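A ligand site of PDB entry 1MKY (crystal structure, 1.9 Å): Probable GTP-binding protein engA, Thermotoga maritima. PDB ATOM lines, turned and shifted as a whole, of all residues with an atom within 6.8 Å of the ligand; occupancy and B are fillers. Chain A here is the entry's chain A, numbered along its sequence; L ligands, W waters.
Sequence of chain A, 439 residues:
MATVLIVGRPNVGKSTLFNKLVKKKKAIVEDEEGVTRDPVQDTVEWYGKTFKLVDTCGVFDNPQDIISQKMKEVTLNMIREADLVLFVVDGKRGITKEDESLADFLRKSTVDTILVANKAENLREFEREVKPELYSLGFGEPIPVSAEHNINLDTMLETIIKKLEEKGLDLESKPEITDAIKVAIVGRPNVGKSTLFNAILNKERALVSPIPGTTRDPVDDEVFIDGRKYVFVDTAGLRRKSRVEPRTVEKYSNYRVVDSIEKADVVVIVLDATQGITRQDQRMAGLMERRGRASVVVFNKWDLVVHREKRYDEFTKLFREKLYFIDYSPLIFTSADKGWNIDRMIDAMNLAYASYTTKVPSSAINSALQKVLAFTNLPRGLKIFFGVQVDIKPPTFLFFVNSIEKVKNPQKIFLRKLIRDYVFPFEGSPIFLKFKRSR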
ATOM      1  N   GLY A 187     -25.428  32.253  28.289  1.00  0.00           N
ATOM      2  CA  GLY A 187     -24.705  31.228  27.561  1.00  0.00           C
ATOM      3  C   GLY A 187     -23.694  31.885  26.647  1.00  0.00           C
ATOM      4  O   GLY A 187     -23.751  33.096  26.413  1.00  0.00           O
ATOM      5  N   ARG A 188     -22.759  31.085  26.140  1.00  0.00           N
ATOM      6  CA  ARG A 188     -21.745  31.613  25.246  1.00  0.00           C
ATOM      7  C   ARG A 188     -22.368  32.081  23.935  1.00  0.00           C
ATOM      8  O   ARG A 188     -23.513  31.737  23.625  1.00  0.00           O
ATOM      9  CB  ARG A 188     -20.673  30.537  24.968  1.00  0.00           C
ATOM     10  CG  ARG A 188     -19.891  30.144  26.210  1.00  0.00           C
ATOM     11  CD  ARG A 188     -18.854  29.058  25.921  1.00  0.00           C
ATOM     12  NE  ARG A 188     -19.440  27.842  25.346  1.00  0.00           N
ATOM     13  CZ  ARG A 188     -19.469  27.564  24.044  1.00  0.00           C
ATOM     14  NH1 ARG A 188     -18.933  28.390  23.159  1.00  0.00           N
ATOM     15  NH2 ARG A 188     -20.050  26.443  23.620  1.00  0.00           N
ATOM     16  N   PRO A 189     -21.642  32.893  23.161  1.00  0.00           N
ATOM     17  CA  PRO A 189     -22.194  33.374  21.896  1.00  0.00           C
ATOM     18  C   PRO A 189     -22.514  32.235  20.932  1.00  0.00           C
ATOM     19  O   PRO A 189     -21.812  31.229  20.905  1.00  0.00           O
ATOM     20  CB  PRO A 189     -21.082  34.272  21.355  1.00  0.00           C
ATOM     21  CG  PRO A 189     -20.533  34.885  22.608  1.00  0.00           C
ATOM     22  CD  PRO A 189     -20.432  33.661  23.533  1.00  0.00           C
ATOM     23  N   ASN A 190     -23.599  32.389  20.189  1.00  0.00           N
ATOM     24  CA  ASN A 190     -24.006  31.409  19.189  1.00  0.00           C
ATOM     25  C   ASN A 190     -24.605  30.101  19.671  1.00  0.00           C
ATOM     26  O   ASN A 190     -24.789  29.182  18.860  1.00  0.00           O
ATOM     27  CB  ASN A 190     -22.829  31.084  18.266  1.00  0.00           C
ATOM     28  CG  ASN A 190     -23.217  31.136  16.810  1.00  0.00           C
ATOM     29  OD1 ASN A 190     -23.492  32.205  16.267  1.00  0.00           O
ATOM     30  ND2 ASN A 190     -23.252  29.964  16.154  1.00  0.00           N
ATOM     31  N   VAL A 191     -24.900  29.978  20.952  1.00  0.00           N
ATOM     32  CA  VAL A 191     -25.476  28.730  21.425  1.00  0.00           C
ATOM     33  C   VAL A 191     -26.966  28.656  21.113  1.00  0.00           C
ATOM     34  O   VAL A 191     -27.548  27.573  21.095  1.00  0.00           O
ATOM     35  CB  VAL A 191     -25.245  28.520  22.951  1.00  0.00           C
ATOM     36  CG1 VAL A 191     -23.756  28.397  23.238  1.00  0.00           C
ATOM     37  CG2 VAL A 191     -25.850  29.669  23.743  1.00  0.00           C
ATOM     38  N   GLY A 192     -27.566  29.810  20.841  1.00  0.00           N
ATOM     39  CA  GLY A 192     -28.984  29.860  20.500  1.00  0.00           C
ATOM     40  C   GLY A 192     -29.887  30.591  21.493  1.00  0.00           C
ATOM     41  O   GLY A 192     -31.091  30.357  21.523  1.00  0.00           O
ATOM     42  N   LYS A 193     -29.299  31.482  22.286  1.00  0.00           N
ATOM     43  CA  LYS A 193     -30.066  32.231  23.278  1.00  0.00           C
ATOM     44  C   LYS A 193     -31.167  33.057  22.640  1.00  0.00           C
ATOM     45  O   LYS A 193     -32.331  32.989  23.049  1.00  0.00           O
ATOM     46  CB  LYS A 193     -29.132  33.153  24.073  1.00  0.00           C
ATOM     47  CG  LYS A 193     -28.040  32.401  24.839  1.00  0.00           C
ATOM     48  CD  LYS A 193     -27.230  33.335  25.736  1.00  0.00           C
ATOM     49  CE  LYS A 193     -26.473  34.399  24.936  1.00  0.00           C
ATOM     50  NZ  LYS A 193     -25.632  33.786  23.871  1.00  0.00           N
ATOM     51  N   SER A 194     -30.803  33.859  21.650  1.00  0.00           N
ATOM     52  CA  SER A 194     -31.771  34.696  20.960  1.00  0.00           C
ATOM     53  C   SER A 194     -32.864  33.861  20.311  1.00  0.00           C
ATOM     54  O   SER A 194     -34.042  34.193  20.420  1.00  0.00           O
ATOM     55  CB  SER A 194     -31.058  35.555  19.899  1.00  0.00           C
ATOM     56  OG  SER A 194     -32.005  36.377  19.236  1.00  0.00           O
ATOM     57  N   THR A 195     -32.477  32.774  19.643  1.00  0.00           N
ATOM     58  CA  THR A 195     -33.456  31.918  18.978  1.00  0.00           C
ATOM     59  C   THR A 195     -34.426  31.272  19.977  1.00  0.00           C
ATOM     60  O   THR A 195     -35.616  31.150  19.704  1.00  0.00           O
ATOM     61  CB  THR A 195     -32.760  30.795  18.155  1.00  0.00           C
ATOM     62  OG1 THR A 195     -31.812  31.378  17.258  1.00  0.00           O
ATOM     63  CG2 THR A 195     -33.773  30.021  17.318  1.00  0.00           C
ATOM     64  N   LEU A 196     -33.899  30.871  21.129  1.00  0.00           N
ATOM     65  CA  LEU A 196     -34.706  30.250  22.174  1.00  0.00           C
ATOM     66  C   LEU A 196     -35.700  31.264  22.773  1.00  0.00           C
ATOM     67  O   LEU A 196     -36.857  30.937  22.999  1.00  0.00           O
ATOM     68  CB  LEU A 196     -33.768  29.725  23.261  1.00  0.00           C
ATOM     69  CG  LEU A 196     -33.977  28.405  23.994  1.00  0.00           C
ATOM     70  CD1 LEU A 196     -34.505  27.291  23.088  1.00  0.00           C
ATOM     71  CD2 LEU A 196     -32.608  28.036  24.603  1.00  0.00           C
ATOM     72  N   GLY A 237     -29.915  41.999  24.068  1.00  0.00           N
ATOM     73  CA  GLY A 237     -29.102  41.061  23.318  1.00  0.00           C
ATOM     74  C   GLY A 237     -29.890  39.940  22.680  1.00  0.00           C
ATOM     75  O   GLY A 237     -29.512  39.422  21.618  1.00  0.00           O
ATOM     76  N   LEU A 238     -30.988  39.546  23.311  1.00  0.00           N
ATOM     77  CA  LEU A 238     -31.828  38.464  22.790  1.00  0.00           C
ATOM     78  C   LEU A 238     -32.798  38.978  21.736  1.00  0.00           C
ATOM     79  O   LEU A 238     -33.235  38.225  20.867  1.00  0.00           O
ATOM     80  CB  LEU A 238     -32.601  37.818  23.944  1.00  0.00           C
ATOM     81  CG  LEU A 238     -31.766  37.290  25.115  1.00  0.00           C
ATOM     82  CD1 LEU A 238     -32.663  36.940  26.285  1.00  0.00           C
ATOM     83  CD2 LEU A 238     -30.954  36.092  24.663  1.00  0.00           C
ATOM     84  N   VAL A 270     -27.798  28.160  28.589  1.00  0.00           N
ATOM     85  CA  VAL A 270     -27.934  27.455  27.325  1.00  0.00           C
ATOM     86  C   VAL A 270     -26.593  26.951  26.834  1.00  0.00           C
ATOM     87  O   VAL A 270     -25.629  27.708  26.729  1.00  0.00           O
ATOM     88  CB  VAL A 270     -28.549  28.403  26.250  1.00  0.00           C
ATOM     89  CG1 VAL A 270     -28.800  27.642  24.966  1.00  0.00           C
ATOM     90  CG2 VAL A 270     -29.848  29.015  26.780  1.00  0.00           C
ATOM     91  N   ASN A 300     -29.109  22.887  23.791  1.00  0.00           N
ATOM     92  CA  ASN A 300     -29.770  23.335  22.584  1.00  0.00           C
ATOM     93  C   ASN A 300     -29.080  22.770  21.332  1.00  0.00           C
ATOM     94  O   ASN A 300     -28.018  22.172  21.431  1.00  0.00           O
ATOM     95  CB  ASN A 300     -29.783  24.869  22.556  1.00  0.00           C
ATOM     96  CG  ASN A 300     -30.649  25.426  21.435  1.00  0.00           C
ATOM     97  OD1 ASN A 300     -31.754  24.934  21.204  1.00  0.00           O
ATOM     98  ND2 ASN A 300     -30.153  26.454  20.740  1.00  0.00           N
ATOM     99  N   LYS A 301     -29.711  22.937  20.171  1.00  0.00           N
ATOM    100  CA  LYS A 301     -29.201  22.431  18.892  1.00  0.00           C
ATOM    101  C   LYS A 301     -29.180  20.908  18.905  1.00  0.00           C
ATOM    102  O   LYS A 301     -28.383  20.258  18.218  1.00  0.00           O
ATOM    103  CB  LYS A 301     -27.798  22.982  18.597  1.00  0.00           C
ATOM    104  CG  LYS A 301     -27.763  24.512  18.535  1.00  0.00           C
ATOM    105  CD  LYS A 301     -26.515  25.052  17.849  1.00  0.00           C
ATOM    106  CE  LYS A 301     -26.417  26.560  17.979  1.00  0.00           C
ATOM    107  NZ  LYS A 301     -25.306  27.131  17.168  1.00  0.00           N
ATOM    108  N   TRP A 302     -30.090  20.345  19.697  1.00  0.00           N
ATOM    109  CA  TRP A 302     -30.218  18.897  19.837  1.00  0.00           C
ATOM    110  C   TRP A 302     -30.487  18.252  18.475  1.00  0.00           C
ATOM    111  O   TRP A 302     -30.152  17.088  18.259  1.00  0.00           O
ATOM    112  CB  TRP A 302     -31.364  18.586  20.805  1.00  0.00           C
ATOM    113  CG  TRP A 302     -31.443  17.138  21.248  1.00  0.00           C
ATOM    114  CD1 TRP A 302     -32.522  16.319  21.160  1.00  0.00           C
ATOM    115  CD2 TRP A 302     -30.404  16.363  21.857  1.00  0.00           C
ATOM    116  NE1 TRP A 302     -32.228  15.083  21.686  1.00  0.00           N
ATOM    117  CE2 TRP A 302     -30.939  15.084  22.117  1.00  0.00           C
ATOM    118  CE3 TRP A 302     -29.073  16.625  22.219  1.00  0.00           C
ATOM    119  CZ2 TRP A 302     -30.194  14.063  22.723  1.00  0.00           C
ATOM    120  CZ3 TRP A 302     -28.324  15.610  22.818  1.00  0.00           C
ATOM    121  CH2 TRP A 302     -28.892  14.350  23.064  1.00  0.00           C
ATOM    122  N   ASP A 303     -31.068  19.021  17.559  1.00  0.00           N
ATOM    123  CA  ASP A 303     -31.374  18.526  16.219  1.00  0.00           C
ATOM    124  C   ASP A 303     -30.111  18.257  15.398  1.00  0.00           C
ATOM    125  O   ASP A 303     -30.156  17.514  14.426  1.00  0.00           O
ATOM    126  CB  ASP A 303     -32.273  19.524  15.475  1.00  0.00           C
ATOM    127  CG  ASP A 303     -31.645  20.901  15.357  1.00  0.00           C
ATOM    128  OD1 ASP A 303     -31.545  21.589  16.394  1.00  0.00           O
ATOM    129  OD2 ASP A 303     -31.260  21.299  14.237  1.00  0.00           O
ATOM    130  N   LEU A 304     -28.995  18.863  15.786  1.00  0.00           N
ATOM    131  CA  LEU A 304     -27.734  18.674  15.072  1.00  0.00           C
ATOM    132  C   LEU A 304     -26.886  17.514  15.615  1.00  0.00           C
ATOM    133  O   LEU A 304     -25.854  17.180  15.029  1.00  0.00           O
ATOM    134  CB  LEU A 304     -26.895  19.950  15.127  1.00  0.00           C
ATOM    135  CG  LEU A 304     -27.470  21.200  14.461  1.00  0.00           C
ATOM    136  CD1 LEU A 304     -26.498  22.364  14.628  1.00  0.00           C
ATOM    137  CD2 LEU A 304     -27.742  20.938  12.997  1.00  0.00           C
ATOM    138  N   THR A 334     -33.269  20.742  23.859  1.00  0.00           N
ATOM    139  CA  THR A 334     -34.074  21.556  22.954  1.00  0.00           C
ATOM    140  C   THR A 334     -33.494  21.781  21.565  1.00  0.00           C
ATOM    141  O   THR A 334     -32.325  21.522  21.303  1.00  0.00           O
ATOM    142  CB  THR A 334     -34.273  22.954  23.514  1.00  0.00           C
ATOM    143  OG1 THR A 334     -33.014  23.651  23.506  1.00  0.00           O
ATOM    144  CG2 THR A 334     -34.800  22.899  24.945  1.00  0.00           C
ATOM    145  N   SER A 335     -34.375  22.284  20.699  1.00  0.00           N
ATOM    146  CA  SER A 335     -34.020  22.693  19.364  1.00  0.00           C
ATOM    147  C   SER A 335     -34.793  23.997  19.200  1.00  0.00           C
ATOM    148  O   SER A 335     -35.992  23.990  18.907  1.00  0.00           O
ATOM    149  CB  SER A 335     -34.467  21.709  18.286  1.00  0.00           C
ATOM    150  OG  SER A 335     -34.104  22.230  17.006  1.00  0.00           O
ATOM    151  N   ALA A 336     -34.111  25.112  19.433  1.00  0.00           N
ATOM    152  CA  ALA A 336     -34.753  26.406  19.299  1.00  0.00           C
ATOM    153  C   ALA A 336     -35.166  26.603  17.854  1.00  0.00           C
ATOM    154  O   ALA A 336     -36.171  27.257  17.564  1.00  0.00           O
ATOM    155  CB  ALA A 336     -33.801  27.504  19.721  1.00  0.00           C
ATOM    156  N   ASP A 337     -34.390  26.012  16.942  1.00  0.00           N
ATOM    157  CA  ASP A 337     -34.654  26.125  15.514  1.00  0.00           C
ATOM    158  C   ASP A 337     -35.917  25.376  15.117  1.00  0.00           C
ATOM    159  O   ASP A 337     -36.808  25.945  14.480  1.00  0.00           O
ATOM    160  CB  ASP A 337     -33.462  25.589  14.729  1.00  0.00           C
ATOM    161  CG  ASP A 337     -33.622  25.796  13.223  1.00  0.00           C
ATOM    162  OD1 ASP A 337     -33.610  26.966  12.781  1.00  0.00           O
ATOM    163  OD2 ASP A 337     -33.758  24.786  12.500  1.00  0.00           O
ATOM    164  N   LYS A 338     -35.997  24.100  15.493  1.00  0.00           N
ATOM    165  CA  LYS A 338     -37.129  23.246  15.170  1.00  0.00           C
ATOM    166  C   LYS A 338     -38.306  23.406  16.123  1.00  0.00           C
ATOM    167  O   LYS A 338     -39.395  22.885  15.861  1.00  0.00           O
ATOM    168  CB  LYS A 338     -36.713  21.766  15.177  1.00  0.00           C
ATOM    169  CG  LYS A 338     -35.501  21.432  14.333  1.00  0.00           C
ATOM    170  CD  LYS A 338     -35.800  21.540  12.857  1.00  0.00           C
ATOM    171  CE  LYS A 338     -34.639  21.036  12.013  1.00  0.00           C
ATOM    172  NZ  LYS A 338     -34.951  21.151  10.563  1.00  0.00           N
ATOM    173  N   GLY A 339     -38.081  24.095  17.237  1.00  0.00           N
ATOM    174  CA  GLY A 339     -39.145  24.282  18.213  1.00  0.00           C
ATOM    175  C   GLY A 339     -39.360  23.002  18.992  1.00  0.00           C
ATOM    176  O   GLY A 339     -40.497  22.553  19.169  1.00  0.00           O
HETATM  177  P1  LIG L   1     -26.922  33.653  20.662  1.00  0.00           P
HETATM  178  O1  LIG L   1     -25.626  34.223  20.233  1.00  0.00           O
HETATM  179  O2  LIG L   1     -27.007  32.678  21.785  1.00  0.00           O
HETATM  180  O3  LIG L   1     -28.060  34.581  21.173  1.00  0.00           O
HETATM  181  O4  LIG L   1     -27.747  32.676  19.874  1.00  0.00           O
HETATM  182  P2  LIG L   1     -28.328  32.888  18.372  1.00  0.00           P
HETATM  183  O5  LIG L   1     -29.725  32.492  18.646  1.00  0.00           O
HETATM  184  O6  LIG L   1     -28.173  34.137  17.622  1.00  0.00           O
HETATM  185  O7  LIG L   1     -28.295  31.425  17.273  1.00  0.00           O
HETATM  186  C1  LIG L   1     -27.060  30.799  16.935  1.00  0.00           C
HETATM  187  C2  LIG L   1     -27.108  30.273  15.489  1.00  0.00           C
HETATM  188  O8  LIG L   1     -27.488  28.850  15.414  1.00  0.00           O
HETATM  189  C3  LIG L   1     -28.176  30.912  14.558  1.00  0.00           C
HETATM  190  O9  LIG L   1     -27.606  30.811  13.228  1.00  0.00           O
HETATM  191  C4  LIG L   1     -29.416  30.009  14.697  1.00  0.00           C
HETATM  192  O10 LIG L   1     -30.247  29.986  13.543  1.00  0.00           O
HETATM  193  C5  LIG L   1     -28.799  28.661  14.969  1.00  0.00           C
HETATM  194  N1  LIG L   1     -29.551  27.914  16.049  1.00  0.00           N
HETATM  195  C6  LIG L   1     -30.037  28.312  17.278  1.00  0.00           C
HETATM  196  N2  LIG L   1     -30.644  27.367  17.918  1.00  0.00           N
HETATM  197  C7  LIG L   1     -30.579  26.257  17.086  1.00  0.00           C
HETATM  198  C8  LIG L   1     -31.056  24.923  17.231  1.00  0.00           C
HETATM  199  O11 LIG L   1     -31.684  24.450  18.183  1.00  0.00           O
HETATM  200  N3  LIG L   1     -30.753  24.106  16.106  1.00  0.00           N
HETATM  201  C9  LIG L   1     -30.055  24.532  14.984  1.00  0.00           C
HETATM  202  N4  LIG L   1     -29.859  23.625  14.023  1.00  0.00           N
HETATM  203  N5  LIG L   1     -29.600  25.798  14.827  1.00  0.00           N
HETATM  204  C10 LIG L   1     -29.898  26.574  15.906  1.00  0.00           C
HETATM  205  O   HOH W   1     -26.485  26.636  14.270  1.00  0.00           O
HETATM  206  O   HOH W   2     -24.469  36.275  20.977  1.00  0.00           O
HETATM  207  O   HOH W   3     -28.555  24.434  11.170  1.00  0.00           O
HETATM  208  O   HOH W   4     -28.423  33.010  11.741  1.00  0.00           O
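The side-chain amino group (NZ) of Lys 193 is in salt-bridge range of an oxygen (O2) of the ligand (2.7 Å).
The backbone NH of Ser 194 sits at hydrogen-bond distance from an oxygen (O3) of the ligand (2.9 Å).
The side-chain hydroxyl (OG1) of Thr 195 is in hydrogen-bond range of an oxygen (O5) of the ligand (2.7 Å).
The side-chain carboxylate of Asp 303 sits at hydrogen-bond distance from a nitrogen (N3) of the ligand, at 2.7 Å.
N of Asp 337 is in hydrogen-bond range of O11 of the ligand (3.4 Å).
The side-chain amino group (NZ) of Lys 301 is in hydrogen-bond range of an oxygen (O8) of the ligand (3.3 Å).
O11 of the ligand lies within hydrogen-bond range of N of Lys 301 (3.2 Å).
ND2 of Asn 300 sits at hydrogen-bond distance from N2 of the ligand (3.0 Å).
The backbone NH (N) of Ala 336 sits at hydrogen-bond distance from an oxygen (O11) of the ligand, at 2.8 Å.
O1 of the ligand is in hydrogen-bond range of N of Asn 190.
N of Gly 192 sits at hydrogen-bond distance from O4 of the ligand, 3.0 Å away.
The side-chain hydroxyl (OG) of Ser 335 sits close to an oxygen (O11) of the ligand (3.5 Å).
N of Thr 195 is in hydrogen-bond range of O5 of the ligand (2.9 Å).
O2 of the ligand lies within hydrogen-bond range of N of Lys 193 (2.6 Å).
ND2 of Asn 300 sits at hydrogen-bond distance from O of Val 191, at 2.9 Å.
The side-chain hydroxyl (OG) of Ser 335 lies within hydrogen-bond range of the backbone NH (N) of Lys 338 (3.1 Å).
OD1 of Asn 300 sits at hydrogen-bond distance from N of Ala 336 (3.0 Å).
The side-chain hydroxyl (OG1) of Thr 334 is in hydrogen-bond range of the side-chain amide oxygen (OD1) of Asn 300 (2.9 Å).
O of Leu 238 lies within hydrogen-bond range of OG of Ser 194.
The side-chain amino group (NZ) of Lys 193 is in hydrogen-bond range of the backbone carbonyl oxygen (O) of Arg 188 (3.0 Å).
The backbone carbonyl oxygen of Gly 187 sits at hydrogen-bond distance from the side-chain amino group of Lys 193, at 3.2 Å.
OG of Ser 335 is in hydrogen-bond range of OD1 of Asp 303.
Pro 189 touches the ligand.
Val 191 touches the ligand (N to O2, 3.5 Å).
Leu 304 touches the ligand.
Hydrophobic or aromatic side chains that line the ligand: Val 191, Leu 304 and Ala 336.
Of the 24 residues printed, 14 come within 4 Å of the ligand.
The nearest printed residue that does not touch the ligand is Arg 188 (4.1 Å).
Water W1 lies within hydrogen-bond range of an oxygen (O8) of the ligand and the side-chain amino group of Lys 301.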
